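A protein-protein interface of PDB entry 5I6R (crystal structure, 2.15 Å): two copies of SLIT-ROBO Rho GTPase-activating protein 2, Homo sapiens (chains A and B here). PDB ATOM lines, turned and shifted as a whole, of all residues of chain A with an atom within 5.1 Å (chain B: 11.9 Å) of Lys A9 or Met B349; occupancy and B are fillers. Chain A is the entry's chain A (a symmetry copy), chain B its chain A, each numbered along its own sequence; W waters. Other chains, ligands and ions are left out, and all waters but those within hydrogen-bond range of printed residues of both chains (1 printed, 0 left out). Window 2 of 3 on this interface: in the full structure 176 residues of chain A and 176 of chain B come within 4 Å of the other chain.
A ring nitrogen (ND1) of His B348 sits at hydrogen-bond distance from the side-chain amide oxygen (OD1) of Asn A171, at 2.8 Å.
N of Met B349 sits at hydrogen-bond distance from O of Lys A8, at 2.7 Å.
OD1 of Asp B351 lies within hydrogen-bond range of N of Ala B353 (2.8 Å).
Among the printed residues, merely in contact across the chains: Phe A7 with Met B349, Lys A9 with Met B349, Lys A8 with Gln B346, Lys A8 with His B348, Ile A175 with Met B349, Asn A171 with Asp B351, Ile A13 with Gln B346, Phe A7 with Gly B350, Ala A172 with Met B349 and Ile A13 with Pro B347.
Of chain B, only Met B349 comes within 4 Å of Lys A9.
Of the printed residues of chain A, Met B349 touches Phe A7 (3.5 Å), Lys A8 (2.7 Å), Lys A9 (3.6 Å), Ala A172 (3.96 Å) and Ile A175 (3.8 Å).
Lys A8 touches just these residues of chain B: Gln B346 (3.6 Å), His B348 (3.7 Å) and Met B349 (2.7 Å).
Asp A10 touches none of the printed residues of chain B.
No residue of chain B comes within 4 Å of Glu A12.
Printed residues of chain A within 4 Å of Gly B350: Phe A7 (3.9 Å).
Of the printed residues of chain B, Ile A175 touches Met B349 (3.8 Å).
Ser B354 touches none of the printed residues of chain A.
The nearest residue of chain B that does not touch Lys A9 is His B348 (4.1 Å).
The nearest printed residue of chain A that does not touch Met B349 is Asn A171 (4.2 Å).
Printed residues of chain B that touch a printed residue of chain A: Gln B346, Pro B347, His B348, Met B349, Gly B350 and Asp B351.
Along chain B the printed residues that touch a printed residue of chain A span positions 346 to 351.
Among the printed residues, 12 pairs touch across the chains.
No position is printed for both chains.
Of the 12 pairs that touch across the chains among the printed residues, none has its exchanged pair printed and touching as well.
Water W1 lies within hydrogen-bond range of N of Asp A10 (3.0 Å) and NE2 of His B348 (3.1 Å).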
ATOM      1  N   PHE A   7     -13.012  -6.698  36.980  1.00  0.00           N
ATOM      2  CA  PHE A   7     -13.195  -7.844  36.073  1.00  0.00           C
ATOM      3  C   PHE A   7     -14.577  -7.640  35.460  1.00  0.00           C
ATOM      4  O   PHE A   7     -15.594  -7.834  36.148  1.00  0.00           O
ATOM      5  CB  PHE A   7     -13.110  -9.160  36.880  1.00  0.00           C
ATOM      6  CG  PHE A   7     -13.586 -10.404  36.150  1.00  0.00           C
ATOM      7  CD1 PHE A   7     -14.948 -10.743  36.095  1.00  0.00           C
ATOM      8  CD2 PHE A   7     -12.664 -11.291  35.582  1.00  0.00           C
ATOM      9  CE1 PHE A   7     -15.375 -11.900  35.444  1.00  0.00           C
ATOM     10  CE2 PHE A   7     -13.088 -12.459  34.944  1.00  0.00           C
ATOM     11  CZ  PHE A   7     -14.444 -12.760  34.874  1.00  0.00           C
ATOM     12  N   LYS A   8     -14.623  -7.234  34.189  1.00  0.00           N
ATOM     13  CA  LYS A   8     -15.884  -6.821  33.578  1.00  0.00           C
ATOM     14  C   LYS A   8     -16.399  -7.791  32.531  1.00  0.00           C
ATOM     15  O   LYS A   8     -15.611  -8.365  31.792  1.00  0.00           O
ATOM     16  CB  LYS A   8     -15.745  -5.415  32.974  1.00  0.00           C
ATOM     17  CG  LYS A   8     -15.496  -4.290  33.973  1.00  0.00           C
ATOM     18  CD  LYS A   8     -15.066  -3.016  33.253  1.00  0.00           C
ATOM     19  CE  LYS A   8     -15.475  -1.774  34.025  1.00  0.00           C
ATOM     20  NZ  LYS A   8     -15.382  -0.547  33.187  1.00  0.00           N
ATOM     21  N   LYS A   9     -17.723  -7.948  32.483  1.00  0.00           N
ATOM     22  CA  LYS A   9     -18.416  -8.783  31.492  1.00  0.00           C
ATOM     23  C   LYS A   9     -19.144  -7.942  30.442  1.00  0.00           C
ATOM     24  O   LYS A   9     -19.110  -6.711  30.493  1.00  0.00           O
ATOM     25  CB  LYS A   9     -19.408  -9.744  32.169  1.00  0.00           C
ATOM     26  CG  LYS A   9     -18.752 -10.846  32.990  1.00  0.00           C
ATOM     27  CD  LYS A   9     -19.567 -12.126  32.980  1.00  0.00           C
ATOM     28  CE  LYS A   9     -18.932 -13.176  33.881  1.00  0.00           C
ATOM     29  NZ  LYS A   9     -19.240 -14.550  33.397  1.00  0.00           N
ATOM     30  N   ASP A  10     -19.810  -8.616  29.504  1.00  0.00           N
ATOM     31  CA  ASP A  10     -20.453  -7.961  28.369  1.00  0.00           C
ATOM     32  C   ASP A  10     -21.495  -6.901  28.734  1.00  0.00           C
ATOM     33  O   ASP A  10     -21.465  -5.804  28.168  1.00  0.00           O
ATOM     34  CB  ASP A  10     -21.057  -8.977  27.402  1.00  0.00           C
ATOM     35  CG  ASP A  10     -21.674  -8.312  26.181  1.00  0.00           C
ATOM     36  OD1 ASP A  10     -20.907  -7.751  25.368  1.00  0.00           O
ATOM     37  OD2 ASP A  10     -22.922  -8.327  26.046  1.00  0.00           O
ATOM     38  N   LYS A  11     -22.413  -7.224  29.653  1.00  0.00           N
ATOM     39  CA  LYS A  11     -23.521  -6.312  30.010  1.00  0.00           C
ATOM     40  C   LYS A  11     -23.050  -4.932  30.503  1.00  0.00           C
ATOM     41  O   LYS A  11     -23.568  -3.904  30.060  1.00  0.00           O
ATOM     42  CB  LYS A  11     -24.497  -6.956  31.007  1.00  0.00           C
ATOM     43  CG  LYS A  11     -25.821  -7.393  30.378  1.00  0.00           C
ATOM     44  CD  LYS A  11     -26.958  -7.521  31.397  1.00  0.00           C
ATOM     45  CE  LYS A  11     -27.535  -6.169  31.823  1.00  0.00           C
ATOM     46  NZ  LYS A  11     -28.792  -6.284  32.618  1.00  0.00           N
ATOM     47  N   GLU A  12     -22.045  -4.943  31.377  1.00  0.00           N
ATOM     48  CA  GLU A  12     -21.475  -3.746  31.973  1.00  0.00           C
ATOM     49  C   GLU A  12     -20.711  -2.908  30.952  1.00  0.00           C
ATOM     50  O   GLU A  12     -20.983  -1.704  30.828  1.00  0.00           O
ATOM     51  CB  GLU A  12     -20.551  -4.123  33.127  1.00  0.00           C
ATOM     52  CG  GLU A  12     -20.354  -3.033  34.166  1.00  0.00           C
ATOM     53  CD  GLU A  12     -19.130  -3.262  35.031  1.00  0.00           C
ATOM     54  OE1 GLU A  12     -18.489  -2.268  35.431  1.00  0.00           O
ATOM     55  OE2 GLU A  12     -18.796  -4.435  35.313  1.00  0.00           O
ATOM     56  N   ILE A  13     -19.768  -3.537  30.231  1.00  0.00           N
ATOM     57  CA  ILE A  13     -18.995  -2.854  29.176  1.00  0.00           C
ATOM     58  C   ILE A  13     -19.936  -2.201  28.148  1.00  0.00           C
ATOM     59  O   ILE A  13     -19.747  -1.031  27.792  1.00  0.00           O
ATOM     60  CB  ILE A  13     -17.927  -3.762  28.507  1.00  0.00           C
ATOM     61  CG1 ILE A  13     -16.898  -4.223  29.548  1.00  0.00           C
ATOM     62  CG2 ILE A  13     -17.184  -3.020  27.393  1.00  0.00           C
ATOM     63  CD1 ILE A  13     -16.147  -5.491  29.176  1.00  0.00           C
ATOM     64  N   ILE A  14     -20.967  -2.933  27.732  1.00  0.00           N
ATOM     65  CA  ILE A  14     -21.925  -2.424  26.754  1.00  0.00           C
ATOM     66  C   ILE A  14     -22.717  -1.248  27.312  1.00  0.00           C
ATOM     67  O   ILE A  14     -22.860  -0.232  26.631  1.00  0.00           O
ATOM     68  CB  ILE A  14     -22.803  -3.556  26.136  1.00  0.00           C
ATOM     69  CG1 ILE A  14     -21.932  -4.507  25.299  1.00  0.00           C
ATOM     70  CG2 ILE A  14     -23.969  -3.031  25.283  1.00  0.00           C
ATOM     71  CD1 ILE A  14     -21.037  -3.846  24.271  1.00  0.00           C
ATOM     72  N   ASN A 171     -13.783 -14.241  23.609  1.00  0.00           N
ATOM     73  CA  ASN A 171     -12.881 -14.237  24.757  1.00  0.00           C
ATOM     74  C   ASN A 171     -13.346 -15.190  25.865  1.00  0.00           C
ATOM     75  O   ASN A 171     -12.513 -15.828  26.527  1.00  0.00           O
ATOM     76  CB  ASN A 171     -12.698 -12.830  25.308  1.00  0.00           C
ATOM     77  CG  ASN A 171     -11.630 -12.756  26.371  1.00  0.00           C
ATOM     78  OD1 ASN A 171     -11.906 -12.410  27.518  1.00  0.00           O
ATOM     79  ND2 ASN A 171     -10.399 -13.094  26.000  1.00  0.00           N
ATOM     80  N   ALA A 172     -14.670 -15.271  26.045  1.00  0.00           N
ATOM     81  CA  ALA A 172     -15.306 -16.140  27.037  1.00  0.00           C
ATOM     82  C   ALA A 172     -15.113 -17.608  26.674  1.00  0.00           C
ATOM     83  O   ALA A 172     -14.762 -18.422  27.538  1.00  0.00           O
ATOM     84  CB  ALA A 172     -16.789 -15.808  27.167  1.00  0.00           C
ATOM     85  N   ILE A 175     -11.598 -18.546  27.450  1.00  0.00           N
ATOM     86  CA  ILE A 175     -11.403 -18.742  28.897  1.00  0.00           C
ATOM     87  C   ILE A 175     -11.925 -20.126  29.371  1.00  0.00           C
ATOM     88  O   ILE A 175     -11.217 -20.844  30.088  1.00  0.00           O
ATOM     89  CB  ILE A 175     -11.977 -17.554  29.725  1.00  0.00           C
ATOM     90  CG1 ILE A 175     -11.073 -16.312  29.568  1.00  0.00           C
ATOM     91  CG2 ILE A 175     -12.114 -17.910  31.208  1.00  0.00           C
ATOM     92  CD1 ILE A 175     -11.625 -15.009  30.130  1.00  0.00           C
ATOM     93  N   PHE B 345      -9.882   1.243  25.108  1.00  0.00           N
ATOM     94  CA  PHE B 345      -9.973  -0.213  25.117  1.00  0.00           C
ATOM     95  C   PHE B 345     -10.436  -0.690  26.490  1.00  0.00           C
ATOM     96  O   PHE B 345      -9.824  -0.336  27.504  1.00  0.00           O
ATOM     97  CB  PHE B 345      -8.623  -0.850  24.743  1.00  0.00           C
ATOM     98  CG  PHE B 345      -8.604  -2.349  24.873  1.00  0.00           C
ATOM     99  CD1 PHE B 345      -9.159  -3.158  23.883  1.00  0.00           C
ATOM    100  CD2 PHE B 345      -8.037  -2.963  26.004  1.00  0.00           C
ATOM    101  CE1 PHE B 345      -9.150  -4.548  24.003  1.00  0.00           C
ATOM    102  CE2 PHE B 345      -8.026  -4.354  26.132  1.00  0.00           C
ATOM    103  CZ  PHE B 345      -8.584  -5.144  25.131  1.00  0.00           C
ATOM    104  N   GLN B 346     -11.530  -1.450  26.505  1.00  0.00           N
ATOM    105  CA  GLN B 346     -12.078  -2.025  27.728  1.00  0.00           C
ATOM    106  C   GLN B 346     -11.789  -3.546  27.832  1.00  0.00           C
ATOM    107  O   GLN B 346     -12.479  -4.357  27.185  1.00  0.00           O
ATOM    108  CB  GLN B 346     -13.585  -1.745  27.844  1.00  0.00           C
ATOM    109  CG  GLN B 346     -13.973  -0.280  28.071  1.00  0.00           C
ATOM    110  CD  GLN B 346     -13.181   0.419  29.181  1.00  0.00           C
ATOM    111  OE1 GLN B 346     -12.609   1.482  28.953  1.00  0.00           O
ATOM    112  NE2 GLN B 346     -13.142  -0.179  30.381  1.00  0.00           N
ATOM    113  N   PRO B 347     -10.771  -3.936  28.642  1.00  0.00           N
ATOM    114  CA  PRO B 347     -10.457  -5.364  28.827  1.00  0.00           C
ATOM    115  C   PRO B 347     -11.659  -6.123  29.347  1.00  0.00           C
ATOM    116  O   PRO B 347     -12.332  -5.654  30.264  1.00  0.00           O
ATOM    117  CB  PRO B 347      -9.345  -5.351  29.877  1.00  0.00           C
ATOM    118  CG  PRO B 347      -8.700  -4.013  29.718  1.00  0.00           C
ATOM    119  CD  PRO B 347      -9.839  -3.079  29.402  1.00  0.00           C
ATOM    120  N   HIS B 348     -11.957  -7.251  28.702  1.00  0.00           N
ATOM    121  CA  HIS B 348     -13.056  -8.145  29.070  1.00  0.00           C
ATOM    122  C   HIS B 348     -12.538  -9.290  29.935  1.00  0.00           C
ATOM    123  O   HIS B 348     -11.476  -9.867  29.648  1.00  0.00           O
ATOM    124  CB  HIS B 348     -13.702  -8.692  27.813  1.00  0.00           C
ATOM    125  CG  HIS B 348     -14.674  -9.809  28.047  1.00  0.00           C
ATOM    126  ND1 HIS B 348     -14.340 -11.136  27.857  1.00  0.00           N
ATOM    127  CD2 HIS B 348     -15.980  -9.795  28.409  1.00  0.00           C
ATOM    128  CE1 HIS B 348     -15.401 -11.887  28.092  1.00  0.00           C
ATOM    129  NE2 HIS B 348     -16.407 -11.100  28.437  1.00  0.00           N
ATOM    130  N   MET B 349     -13.284  -9.586  31.002  1.00  0.00           N
ATOM    131  CA  MET B 349     -12.960 -10.651  31.950  1.00  0.00           C
ATOM    132  C   MET B 349     -11.455 -10.732  32.241  1.00  0.00           C
ATOM    133  O   MET B 349     -10.842 -11.778  32.074  1.00  0.00           O
ATOM    134  CB  MET B 349     -13.481 -12.008  31.435  1.00  0.00           C
ATOM    135  CG  MET B 349     -14.999 -12.207  31.446  1.00  0.00           C
ATOM    136  SD  MET B 349     -15.426 -13.871  30.864  1.00  0.00           S
ATOM    137  CE  MET B 349     -17.197 -13.793  30.554  1.00  0.00           C
ATOM    138  N   GLY B 350     -10.857  -9.608  32.620  1.00  0.00           N
ATOM    139  CA  GLY B 350      -9.458  -9.564  33.056  1.00  0.00           C
ATOM    140  C   GLY B 350      -8.368  -9.692  32.007  1.00  0.00           C
ATOM    141  O   GLY B 350      -7.210  -9.977  32.356  1.00  0.00           O
ATOM    142  N   ASP B 351      -8.720  -9.460  30.737  1.00  0.00           N
ATOM    143  CA  ASP B 351      -7.782  -9.584  29.610  1.00  0.00           C
ATOM    144  C   ASP B 351      -6.535  -8.716  29.800  1.00  0.00           C
ATOM    145  O   ASP B 351      -6.631  -7.520  30.056  1.00  0.00           O
ATOM    146  CB  ASP B 351      -8.494  -9.253  28.290  1.00  0.00           C
ATOM    147  CG  ASP B 351      -7.701  -9.675  27.041  1.00  0.00           C
ATOM    148  OD1 ASP B 351      -6.448  -9.752  27.058  1.00  0.00           O
ATOM    149  OD2 ASP B 351      -8.360  -9.900  26.007  1.00  0.00           O
ATOM    150  N   MET B 352      -5.381  -9.359  29.662  1.00  0.00           N
ATOM    151  CA  MET B 352      -4.035  -8.797  29.842  1.00  0.00           C
ATOM    152  C   MET B 352      -3.545  -8.012  28.626  1.00  0.00           C
ATOM    153  O   MET B 352      -2.678  -7.144  28.730  1.00  0.00           O
ATOM    154  CB  MET B 352      -3.037  -9.946  30.143  1.00  0.00           C
ATOM    155  CG  MET B 352      -3.092 -11.138  29.170  1.00  0.00           C
ATOM    156  SD  MET B 352      -2.051 -12.569  29.549  1.00  0.00           S
ATOM    157  CE  MET B 352      -2.598 -13.726  28.296  1.00  0.00           C
ATOM    158  N   ALA B 353      -4.058  -8.387  27.457  1.00  0.00           N
ATOM    159  CA  ALA B 353      -3.597  -7.805  26.195  1.00  0.00           C
ATOM    160  C   ALA B 353      -4.384  -6.546  25.829  1.00  0.00           C
ATOM    161  O   ALA B 353      -5.590  -6.470  26.059  1.00  0.00           O
ATOM    162  CB  ALA B 353      -3.639  -8.836  25.071  1.00  0.00           C
ATOM    163  N   SER B 354      -3.680  -5.564  25.272  1.00  0.00           N
ATOM    164  CA  SER B 354      -4.245  -4.250  24.965  1.00  0.00           C
ATOM    165  C   SER B 354      -3.830  -3.736  23.572  1.00  0.00           C
ATOM    166  O   SER B 354      -4.277  -2.676  23.146  1.00  0.00           O
ATOM    167  CB  SER B 354      -3.819  -3.249  26.045  1.00  0.00           C
ATOM    168  OG  SER B 354      -2.403  -3.099  26.056  1.00  0.00           O
HETATM  169  O   HOH W   1     -19.346 -11.565  29.249  1.00  0.00           O
